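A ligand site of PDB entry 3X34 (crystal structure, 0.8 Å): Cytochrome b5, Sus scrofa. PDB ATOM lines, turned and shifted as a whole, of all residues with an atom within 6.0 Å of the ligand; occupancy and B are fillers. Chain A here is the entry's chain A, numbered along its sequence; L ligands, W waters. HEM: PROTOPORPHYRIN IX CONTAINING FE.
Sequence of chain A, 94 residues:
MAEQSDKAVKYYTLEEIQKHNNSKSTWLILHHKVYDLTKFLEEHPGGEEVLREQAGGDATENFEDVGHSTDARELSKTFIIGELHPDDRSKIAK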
ATOM      1  N   LEU A  28     -11.457 -34.017 -14.690  1.00  0.00           N
ATOM      2  CA  LEU A  28     -10.229 -33.324 -15.122  1.00  0.00           C
ATOM      3  C   LEU A  28      -9.046 -33.917 -14.338  1.00  0.00           C
ATOM      4  O   LEU A  28      -9.237 -34.372 -13.212  1.00  0.00           O
ATOM      5  CB  LEU A  28     -10.186 -31.814 -14.949  1.00  0.00           C
ATOM      6  CG  LEU A  28     -10.940 -30.974 -15.983  1.00  0.00           C
ATOM      7  CD1 LEU A  28     -12.438 -31.229 -16.008  1.00  0.00           C
ATOM      8  CD2 LEU A  28     -10.635 -29.496 -15.807  1.00  0.00           C
ATOM      9  N   LEU A  30      -5.250 -32.852 -12.941  1.00  0.00           N
ATOM     10  CA  LEU A  30      -4.300 -31.781 -12.639  1.00  0.00           C
ATOM     11  C   LEU A  30      -3.147 -32.424 -11.882  1.00  0.00           C
ATOM     12  O   LEU A  30      -3.373 -33.056 -10.827  1.00  0.00           O
ATOM     13  CB  LEU A  30      -4.857 -30.647 -11.774  1.00  0.00           C
ATOM     14  CG  LEU A  30      -6.140 -29.985 -12.284  1.00  0.00           C
ATOM     15  CD1 LEU A  30      -6.719 -29.081 -11.227  1.00  0.00           C
ATOM     16  CD2 LEU A  30      -5.894 -29.221 -13.579  1.00  0.00           C
ATOM     17  N   TYR A  35      -9.928 -35.044 -10.611  1.00  0.00           N
ATOM     18  CA  TYR A  35     -10.902 -34.162  -9.977  1.00  0.00           C
ATOM     19  C   TYR A  35     -12.260 -34.366 -10.612  1.00  0.00           C
ATOM     20  O   TYR A  35     -12.391 -34.318 -11.837  1.00  0.00           O
ATOM     21  CB  TYR A  35     -10.481 -32.672 -10.232  1.00  0.00           C
ATOM     22  CG  TYR A  35      -9.172 -32.311  -9.584  1.00  0.00           C
ATOM     23  CD1 TYR A  35      -7.956 -32.755 -10.086  1.00  0.00           C
ATOM     24  CD2 TYR A  35      -9.152 -31.511  -8.445  1.00  0.00           C
ATOM     25  CE1 TYR A  35      -6.775 -32.475  -9.450  1.00  0.00           C
ATOM     26  CE2 TYR A  35      -7.938 -31.175  -7.828  1.00  0.00           C
ATOM     27  CZ  TYR A  35      -6.762 -31.666  -8.330  1.00  0.00           C
ATOM     28  OH  TYR A  35      -5.573 -31.397  -7.698  1.00  0.00           O
ATOM     29  N   LEU A  37     -15.423 -32.628 -11.273  1.00  0.00           N
ATOM     30  CA  LEU A  37     -15.964 -31.275 -11.336  1.00  0.00           C
ATOM     31  C   LEU A  37     -17.396 -31.238 -11.866  1.00  0.00           C
ATOM     32  O   LEU A  37     -17.901 -30.173 -12.225  1.00  0.00           O
ATOM     33  CB  LEU A  37     -15.057 -30.343 -12.155  1.00  0.00           C
ATOM     34  CG  LEU A  37     -13.603 -30.294 -11.652  1.00  0.00           C
ATOM     35  CD1 LEU A  37     -12.853 -29.244 -12.439  1.00  0.00           C
ATOM     36  CD2 LEU A  37     -13.501 -30.038 -10.170  1.00  0.00           C
ATOM     37  N   PHE A  40     -19.177 -28.886  -9.532  1.00  0.00           N
ATOM     38  CA  PHE A  40     -18.443 -27.647  -9.341  1.00  0.00           C
ATOM     39  C   PHE A  40     -18.486 -26.769 -10.576  1.00  0.00           C
ATOM     40  O   PHE A  40     -18.499 -25.522 -10.447  1.00  0.00           O
ATOM     41  CB  PHE A  40     -16.977 -27.947  -8.975  1.00  0.00           C
ATOM     42  CG  PHE A  40     -16.195 -26.650  -8.865  1.00  0.00           C
ATOM     43  CD1 PHE A  40     -16.457 -25.749  -7.867  1.00  0.00           C
ATOM     44  CD2 PHE A  40     -15.201 -26.346  -9.813  1.00  0.00           C
ATOM     45  CE1 PHE A  40     -15.783 -24.528  -7.801  1.00  0.00           C
ATOM     46  CE2 PHE A  40     -14.528 -25.145  -9.746  1.00  0.00           C
ATOM     47  CZ  PHE A  40     -14.823 -24.252  -8.742  1.00  0.00           C
ATOM     48  N   HIS A  44     -18.171 -22.592 -10.903  1.00  0.00           N
ATOM     49  CA  HIS A  44     -16.801 -22.137 -11.097  1.00  0.00           C
ATOM     50  C   HIS A  44     -16.777 -20.680 -11.508  1.00  0.00           C
ATOM     51  O   HIS A  44     -17.378 -20.318 -12.546  1.00  0.00           O
ATOM     52  CB  HIS A  44     -16.198 -22.989 -12.213  1.00  0.00           C
ATOM     53  CG  HIS A  44     -14.798 -22.576 -12.573  1.00  0.00           C
ATOM     54  ND1 HIS A  44     -14.396 -22.411 -13.877  1.00  0.00           N
ATOM     55  CD2 HIS A  44     -13.688 -22.375 -11.799  1.00  0.00           C
ATOM     56  CE1 HIS A  44     -13.072 -22.140 -13.849  1.00  0.00           C
ATOM     57  NE2 HIS A  44     -12.619 -22.095 -12.626  1.00  0.00           N
ATOM     58  N   PRO A  45     -16.032 -19.803 -10.843  1.00  0.00           N
ATOM     59  CA  PRO A  45     -16.007 -18.387 -11.263  1.00  0.00           C
ATOM     60  C   PRO A  45     -15.449 -18.185 -12.653  1.00  0.00           C
ATOM     61  O   PRO A  45     -15.877 -17.203 -13.329  1.00  0.00           O
ATOM     62  CB  PRO A  45     -15.118 -17.748 -10.163  1.00  0.00           C
ATOM     63  CG  PRO A  45     -15.358 -18.534  -8.969  1.00  0.00           C
ATOM     64  CD  PRO A  45     -15.433 -19.990  -9.496  1.00  0.00           C
ATOM     65  N   GLY A  46     -14.580 -19.022 -13.143  1.00  0.00           N
ATOM     66  CA  GLY A  46     -14.107 -18.912 -14.520  1.00  0.00           C
ATOM     67  C   GLY A  46     -15.066 -19.412 -15.597  1.00  0.00           C
ATOM     68  O   GLY A  46     -14.714 -19.381 -16.780  1.00  0.00           O
ATOM     69  N   GLY A  47     -16.251 -19.869 -15.191  1.00  0.00           N
ATOM     70  CA  GLY A  47     -17.283 -20.275 -16.119  1.00  0.00           C
ATOM     71  C   GLY A  47     -17.222 -21.767 -16.408  1.00  0.00           C
ATOM     72  O   GLY A  47     -16.309 -22.499 -16.008  1.00  0.00           O
ATOM     73  N   VAL A  50     -14.893 -23.242 -20.064  1.00  0.00           N
ATOM     74  CA  VAL A  50     -13.465 -23.404 -19.943  1.00  0.00           C
ATOM     75  C   VAL A  50     -13.119 -24.751 -19.336  1.00  0.00           C
ATOM     76  O   VAL A  50     -12.105 -25.390 -19.664  1.00  0.00           O
ATOM     77  CB  VAL A  50     -12.839 -22.229 -19.145  1.00  0.00           C
ATOM     78  CG1 VAL A  50     -12.971 -22.333 -17.628  1.00  0.00           C
ATOM     79  CG2 VAL A  50     -11.340 -22.149 -19.428  1.00  0.00           C
ATOM     80  N   LEU A  51     -13.971 -25.363 -18.422  1.00  0.00           N
ATOM     81  CA  LEU A  51     -13.879 -26.678 -17.821  1.00  0.00           C
ATOM     82  C   LEU A  51     -14.420 -27.764 -18.753  1.00  0.00           C
ATOM     83  O   LEU A  51     -13.812 -28.832 -18.896  1.00  0.00           O
ATOM     84  CB  LEU A  51     -14.583 -26.719 -16.462  1.00  0.00           C
ATOM     85  CG  LEU A  51     -14.031 -25.725 -15.429  1.00  0.00           C
ATOM     86  CD1 LEU A  51     -14.809 -25.867 -14.129  1.00  0.00           C
ATOM     87  CD2 LEU A  51     -12.571 -25.886 -15.191  1.00  0.00           C
ATOM     88  N   GLN A  54     -12.007 -29.117 -21.241  1.00  0.00           N
ATOM     89  CA  GLN A  54     -10.975 -29.952 -20.668  1.00  0.00           C
ATOM     90  C   GLN A  54     -11.476 -31.330 -20.185  1.00  0.00           C
ATOM     91  O   GLN A  54     -10.675 -32.165 -19.803  1.00  0.00           O
ATOM     92  CB  GLN A  54     -10.332 -29.250 -19.469  1.00  0.00           C
ATOM     93  CG  GLN A  54      -9.684 -27.943 -19.828  1.00  0.00           C
ATOM     94  CD  GLN A  54      -8.578 -28.102 -20.851  1.00  0.00           C
ATOM     95  OE1 GLN A  54      -7.818 -29.077 -20.761  1.00  0.00           O
ATOM     96  NE2 GLN A  54      -8.508 -27.192 -21.798  1.00  0.00           N
ATOM     97  N   ALA A  59      -5.677 -30.876 -17.610  1.00  0.00           N
ATOM     98  CA  ALA A  59      -5.837 -29.437 -17.691  1.00  0.00           C
ATOM     99  C   ALA A  59      -4.796 -28.697 -16.845  1.00  0.00           C
ATOM    100  O   ALA A  59      -5.008 -27.529 -16.496  1.00  0.00           O
ATOM    101  CB  ALA A  59      -7.248 -29.044 -17.260  1.00  0.00           C
ATOM    102  N   ASN A  62      -3.445 -25.243 -18.156  1.00  0.00           N
ATOM    103  CA  ASN A  62      -4.469 -24.225 -18.159  1.00  0.00           C
ATOM    104  C   ASN A  62      -4.721 -23.702 -16.730  1.00  0.00           C
ATOM    105  O   ASN A  62      -4.850 -22.514 -16.499  1.00  0.00           O
ATOM    106  CB  ASN A  62      -5.771 -24.742 -18.745  1.00  0.00           C
ATOM    107  CG  ASN A  62      -5.597 -25.495 -20.033  1.00  0.00           C
ATOM    108  OD1 ASN A  62      -4.988 -26.577 -20.020  1.00  0.00           O
ATOM    109  ND2 ASN A  62      -6.068 -24.936 -21.112  1.00  0.00           N
ATOM    110  N   PHE A  63      -4.834 -24.650 -15.794  1.00  0.00           N
ATOM    111  CA  PHE A  63      -5.062 -24.295 -14.408  1.00  0.00           C
ATOM    112  C   PHE A  63      -3.945 -23.412 -13.851  1.00  0.00           C
ATOM    113  O   PHE A  63      -4.181 -22.400 -13.193  1.00  0.00           O
ATOM    114  CB  PHE A  63      -5.181 -25.577 -13.578  1.00  0.00           C
ATOM    115  CG  PHE A  63      -5.386 -25.324 -12.086  1.00  0.00           C
ATOM    116  CD1 PHE A  63      -4.321 -25.362 -11.220  1.00  0.00           C
ATOM    117  CD2 PHE A  63      -6.644 -25.059 -11.597  1.00  0.00           C
ATOM    118  CE1 PHE A  63      -4.509 -25.085  -9.870  1.00  0.00           C
ATOM    119  CE2 PHE A  63      -6.857 -24.810 -10.244  1.00  0.00           C
ATOM    120  CZ  PHE A  63      -5.785 -24.769  -9.386  1.00  0.00           C
ATOM    121  N   VAL A  66      -3.757 -20.061 -15.642  1.00  0.00           N
ATOM    122  CA  VAL A  66      -4.758 -19.072 -15.245  1.00  0.00           C
ATOM    123  C   VAL A  66      -4.304 -18.188 -14.103  1.00  0.00           C
ATOM    124  O   VAL A  66      -4.721 -17.025 -14.056  1.00  0.00           O
ATOM    125  CB  VAL A  66      -6.060 -19.788 -14.799  1.00  0.00           C
ATOM    126  CG1 VAL A  66      -7.054 -18.966 -13.996  1.00  0.00           C
ATOM    127  CG2 VAL A  66      -6.736 -20.272 -16.064  1.00  0.00           C
ATOM    128  N   GLY A  67      -3.482 -18.777 -13.118  1.00  0.00           N
ATOM    129  CA  GLY A  67      -3.133 -18.052 -11.939  1.00  0.00           C
ATOM    130  C   GLY A  67      -4.154 -17.998 -10.793  1.00  0.00           C
ATOM    131  O   GLY A  67      -4.571 -16.909 -10.410  1.00  0.00           O
ATOM    132  N   HIS A  68      -4.573 -19.081 -10.048  1.00  0.00           N
ATOM    133  CA  HIS A  68      -5.614 -19.297  -9.084  1.00  0.00           C
ATOM    134  C   HIS A  68      -5.113 -18.914  -7.687  1.00  0.00           C
ATOM    135  O   HIS A  68      -3.931 -19.167  -7.302  1.00  0.00           O
ATOM    136  CB  HIS A  68      -6.026 -20.795  -9.075  1.00  0.00           C
ATOM    137  CG  HIS A  68      -6.972 -21.159 -10.190  1.00  0.00           C
ATOM    138  ND1 HIS A  68      -6.607 -21.592 -11.446  1.00  0.00           N
ATOM    139  CD2 HIS A  68      -8.342 -21.125 -10.241  1.00  0.00           C
ATOM    140  CE1 HIS A  68      -7.710 -21.815 -12.145  1.00  0.00           C
ATOM    141  NE2 HIS A  68      -8.799 -21.543 -11.458  1.00  0.00           N
ATOM    142  N   SER A  69      -6.008 -18.363  -6.877  1.00  0.00           N
ATOM    143  CA  SER A  69      -5.704 -17.985  -5.498  1.00  0.00           C
ATOM    144  C   SER A  69      -5.393 -19.198  -4.619  1.00  0.00           C
ATOM    145  O   SER A  69      -5.752 -20.326  -4.970  1.00  0.00           O
ATOM    146  CB  SER A  69      -6.862 -17.197  -4.947  1.00  0.00           C
ATOM    147  OG  SER A  69      -8.002 -18.064  -4.733  1.00  0.00           O
ATOM    148  N   ASP A  71      -6.920 -19.783  -1.889  1.00  0.00           N
ATOM    149  CA  ASP A  71      -8.263 -20.322  -1.514  1.00  0.00           C
ATOM    150  C   ASP A  71      -8.775 -21.201  -2.662  1.00  0.00           C
ATOM    151  O   ASP A  71      -9.381 -22.259  -2.384  1.00  0.00           O
ATOM    152  CB  ASP A  71      -9.221 -19.211  -1.179  1.00  0.00           C
ATOM    153  CG  ASP A  71      -9.051 -18.607   0.225  1.00  0.00           C
ATOM    154  OD1 ASP A  71      -8.118 -19.126   1.021  1.00  0.00           O
ATOM    155  OD2 ASP A  71      -9.794 -17.776   0.579  1.00  0.00           O
ATOM    156  N   ALA A  72      -8.593 -20.810  -3.913  1.00  0.00           N
ATOM    157  CA  ALA A  72      -9.039 -21.641  -5.029  1.00  0.00           C
ATOM    158  C   ALA A  72      -8.269 -22.986  -5.072  1.00  0.00           C
ATOM    159  O   ALA A  72      -8.853 -24.024  -5.336  1.00  0.00           O
ATOM    160  CB  ALA A  72      -8.905 -20.892  -6.370  1.00  0.00           C
ATOM    161  N   ARG A  73      -6.958 -22.899  -4.992  1.00  0.00           N
ATOM    162  CA  ARG A  73      -6.177 -24.103  -5.029  1.00  0.00           C
ATOM    163  C   ARG A  73      -6.598 -25.039  -3.872  1.00  0.00           C
ATOM    164  O   ARG A  73      -6.757 -26.266  -4.045  1.00  0.00           O
ATOM    165  CB  ARG A  73      -4.689 -23.767  -4.927  1.00  0.00           C
ATOM    166  CG  ARG A  73      -3.802 -24.939  -5.324  1.00  0.00           C
ATOM    167  CD  ARG A  73      -2.320 -24.550  -5.300  1.00  0.00           C
ATOM    168  NE  ARG A  73      -1.967 -23.686  -6.342  1.00  0.00           N
ATOM    169  CZ  ARG A  73      -1.466 -24.012  -7.526  1.00  0.00           C
ATOM    170  NH1 ARG A  73      -1.239 -25.271  -7.864  1.00  0.00           N
ATOM    171  NH2 ARG A  73      -1.197 -23.063  -8.413  1.00  0.00           N
ATOM    172  N   LEU A  75      -9.692 -25.131  -2.393  1.00  0.00           N
ATOM    173  CA  LEU A  75     -11.005 -25.570  -2.835  1.00  0.00           C
ATOM    174  C   LEU A  75     -10.841 -26.733  -3.825  1.00  0.00           C
ATOM    175  O   LEU A  75     -11.599 -27.720  -3.757  1.00  0.00           O
ATOM    176  CB  LEU A  75     -11.770 -24.400  -3.456  1.00  0.00           C
ATOM    177  CG  LEU A  75     -13.117 -24.697  -4.013  1.00  0.00           C
ATOM    178  CD1 LEU A  75     -14.086 -25.256  -2.981  1.00  0.00           C
ATOM    179  CD2 LEU A  75     -13.688 -23.435  -4.652  1.00  0.00           C
ATOM    180  N   SER A  76      -9.897 -26.645  -4.745  1.00  0.00           N
ATOM    181  CA  SER A  76      -9.731 -27.715  -5.710  1.00  0.00           C
ATOM    182  C   SER A  76      -9.521 -29.068  -5.083  1.00  0.00           C
ATOM    183  O   SER A  76      -9.986 -30.084  -5.603  1.00  0.00           O
ATOM    184  CB  SER A  76      -8.590 -27.399  -6.704  1.00  0.00           C
ATOM    185  OG  SER A  76      -7.316 -27.552  -6.170  1.00  0.00           O
ATOM    186  N   LYS A  77      -8.792 -29.099  -3.961  1.00  0.00           N
ATOM    187  CA  LYS A  77      -8.485 -30.357  -3.320  1.00  0.00           C
ATOM    188  C   LYS A  77      -9.707 -31.092  -2.888  1.00  0.00           C
ATOM    189  O   LYS A  77      -9.703 -32.344  -2.792  1.00  0.00           O
ATOM    190  CB  LYS A  77      -7.534 -30.069  -2.147  1.00  0.00           C
ATOM    191  CG  LYS A  77      -6.283 -29.346  -2.658  1.00  0.00           C
ATOM    192  CD  LYS A  77      -4.989 -29.701  -2.020  1.00  0.00           C
ATOM    193  CE  LYS A  77      -4.041 -28.658  -1.517  1.00  0.00           C
ATOM    194  NZ  LYS A  77      -3.755 -28.684  -0.057  1.00  0.00           N
ATOM    195  N   PHE A  79     -12.300 -31.707  -4.479  1.00  0.00           N
ATOM    196  CA  PHE A  79     -12.869 -32.448  -5.600  1.00  0.00           C
ATOM    197  C   PHE A  79     -11.982 -33.595  -6.054  1.00  0.00           C
ATOM    198  O   PHE A  79     -12.351 -34.295  -7.016  1.00  0.00           O
ATOM    199  CB  PHE A  79     -13.151 -31.502  -6.772  1.00  0.00           C
ATOM    200  CG  PHE A  79     -14.095 -30.377  -6.389  1.00  0.00           C
ATOM    201  CD1 PHE A  79     -15.435 -30.666  -6.132  1.00  0.00           C
ATOM    202  CD2 PHE A  79     -13.678 -29.088  -6.275  1.00  0.00           C
ATOM    203  CE1 PHE A  79     -16.271 -29.666  -5.691  1.00  0.00           C
ATOM    204  CE2 PHE A  79     -14.546 -28.071  -5.887  1.00  0.00           C
ATOM    205  CZ  PHE A  79     -15.853 -28.377  -5.578  1.00  0.00           C
HETATM  206  CHA HEM L   1     -11.183 -18.449 -11.669  1.00  0.00           C
HETATM  207  CHB HEM L   1     -11.634 -22.273  -8.783  1.00  0.00           C
HETATM  208  CHC HEM L   1     -10.077 -25.130 -12.304  1.00  0.00           C
HETATM  209  CHD HEM L   1      -9.931 -21.364 -15.309  1.00  0.00           C
HETATM  210  C1A HEM L   1     -11.379 -19.228 -10.551  1.00  0.00           C
HETATM  211  C2A HEM L   1     -11.744 -18.729  -9.244  1.00  0.00           C
HETATM  212  C3A HEM L   1     -11.945 -19.814  -8.434  1.00  0.00           C
HETATM  213  C4A HEM L   1     -11.666 -20.980  -9.268  1.00  0.00           C
HETATM  214  CMA HEM L   1     -12.406 -19.870  -7.022  1.00  0.00           C
HETATM  215  CAA HEM L   1     -11.825 -17.266  -8.866  1.00  0.00           C
HETATM  216  CBA HEM L   1     -10.466 -16.596  -8.761  1.00  0.00           C
HETATM  217  CGA HEM L   1      -9.510 -17.284  -7.743  1.00  0.00           C
HETATM  218  O1A HEM L   1      -9.858 -17.439  -6.587  1.00  0.00           O
HETATM  219  O2A HEM L   1      -8.382 -17.623  -8.178  1.00  0.00           O
HETATM  220  C1B HEM L   1     -11.248 -23.394  -9.493  1.00  0.00           C
HETATM  221  C2B HEM L   1     -11.213 -24.720  -8.942  1.00  0.00           C
HETATM  222  C3B HEM L   1     -10.691 -25.543  -9.857  1.00  0.00           C
HETATM  223  C4B HEM L   1     -10.534 -24.683 -11.084  1.00  0.00           C
HETATM  224  CMB HEM L   1     -11.572 -25.057  -7.514  1.00  0.00           C
HETATM  225  CAB HEM L   1     -10.255 -26.960  -9.906  1.00  0.00           C
HETATM  226  CBB HEM L   1     -10.900 -27.903  -9.263  1.00  0.00           C
HETATM  227  C1C HEM L   1      -9.848 -24.334 -13.428  1.00  0.00           C
HETATM  228  C2C HEM L   1      -9.365 -24.859 -14.688  1.00  0.00           C
HETATM  229  C3C HEM L   1      -9.348 -23.795 -15.555  1.00  0.00           C
HETATM  230  C4C HEM L   1      -9.806 -22.650 -14.791  1.00  0.00           C
HETATM  231  CMC HEM L   1      -8.919 -26.285 -14.907  1.00  0.00           C
HETATM  232  CAC HEM L   1      -9.013 -23.787 -16.960  1.00  0.00           C
HETATM  233  CBC HEM L   1      -9.215 -24.811 -17.800  1.00  0.00           C
HETATM  234  C1D HEM L   1     -10.317 -20.242 -14.599  1.00  0.00           C
HETATM  235  C2D HEM L   1     -10.378 -18.905 -15.161  1.00  0.00           C
HETATM  236  C3D HEM L   1     -10.729 -18.085 -14.138  1.00  0.00           C
HETATM  237  C4D HEM L   1     -10.840 -18.932 -12.933  1.00  0.00           C
HETATM  238  CMD HEM L   1     -10.158 -18.568 -16.602  1.00  0.00           C
HETATM  239  CAD HEM L   1     -10.614 -16.560 -13.955  1.00  0.00           C
HETATM  240  CBD HEM L   1     -11.916 -15.935 -14.354  1.00  0.00           C
HETATM  241  CGD HEM L   1     -11.896 -14.408 -14.503  1.00  0.00           C
HETATM  242  O1D HEM L   1     -11.721 -13.894 -15.659  1.00  0.00           O
HETATM  243  O2D HEM L   1     -12.065 -13.715 -13.478  1.00  0.00           O
HETATM  244  NA  HEM L   1     -11.310 -20.607 -10.542  1.00  0.00           N
HETATM  245  NB  HEM L   1     -10.840 -23.381 -10.789  1.00  0.00           N
HETATM  246  NC  HEM L   1     -10.102 -22.999 -13.513  1.00  0.00           N
HETATM  247  ND  HEM L   1     -10.613 -20.230 -13.258  1.00  0.00           N
HETATM  248 FE   HEM L   1     -10.712 -21.802 -12.030  1.00  0.00          FE
HETATM  249  O   HOH W   1     -14.674 -14.638 -13.846  1.00  0.00           O
HETATM  250  O   HOH W   2      -9.111 -14.064 -16.685  1.00  0.00           O
HETATM  251  O   HOH W   3     -11.264 -17.684  -3.694  1.00  0.00           O
HETATM  252  O   HOH W   4      -7.979 -17.686 -10.726  1.00  0.00           O
HETATM  253  O   HOH W   5     -12.240 -20.108  -3.646  1.00  0.00           O
HETATM  254  O   HOH W   6     -12.121 -11.320 -12.502  1.00  0.00           O
HETATM  255  O   HOH W   7     -11.676 -15.935  -5.370  1.00  0.00           O
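The backbone carbonyl oxygen (O) of Phe 63 lies within hydrogen-bond range of a ring nitrogen (ND1) of His 68, 3.1 Å away.
A ring nitrogen (ND1) of His 44 sits close to the backbone NH (N) of Gly 46 (3.5 Å).
O of Gly 47 is in hydrogen-bond range of ND1 of His 44 (2.9 Å).
The side-chain hydroxyl (OG) of Ser 69 lies within hydrogen-bond range of the backbone NH (N) of Ala 72, at 2.9 Å.
OG of Ser 69 lies close to N of Asp 71.
OG of Ser 76 is in hydrogen-bond range of O of Arg 73 (2.5 Å).
The side-chain amide nitrogen (ND2) of Asn 62 sits close to the side-chain amide nitrogen (NE2) of Gln 54, 3.4 Å away.
The backbone carbonyl oxygen (O) of Leu 28 is in hydrogen-bond range of the backbone NH (N) of Tyr 35, 2.8 Å away.
Residues that only touch the ligand: Leu 28 (3.8 Å), Leu 37 (3.5 Å), Phe 40 (3.4 Å), Pro 45 (3.6 Å), Gly 46 (3.5 Å), Val 50 (3.5 Å), Leu 51 (3.4 Å), Gln 54 (3.8 Å), Ala 59 (3.99 Å), Asn 62 (3.6 Å), Phe 63 (3.5 Å), Val 66 (3.5 Å), Ala 72 (3.6 Å), Leu 75 (3.8 Å) and Ser 76 (3.5 Å).
Within 4 Å of the ligand: Leu 28, Leu 37, Phe 40, His 44, Pro 45, Gly 46, Val 50, Leu 51, Gln 54, Ala 59, Asn 62, Phe 63, Val 66, His 68, Ser 69, Ala 72, Leu 75 and Ser 76.
The nearest printed residue that does not touch the ligand is Tyr 35 (4.1 Å).
Water W1 lies within hydrogen-bond range of O2D of the ligand and O of Pro 45.
Water W3 lies within hydrogen-bond range of an oxygen (O1A) of the ligand (3.2 Å) and the side-chain hydroxyl (OG) of Ser 69 (3.4 Å).
A ring nitrogen (NE2) of His 68 binds an iron atom (FE) of the ligand (2.0 Å).
A ring nitrogen (NE2) of His 44 is bound to an iron atom (FE) of the ligand.
O2A of the ligand is in hydrogen-bond range of N of Ser 69 (2.8 Å).
An oxygen (O1A) of the ligand lies within hydrogen-bond range of the side-chain hydroxyl (OG) of Ser 69 (2.7 Å).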
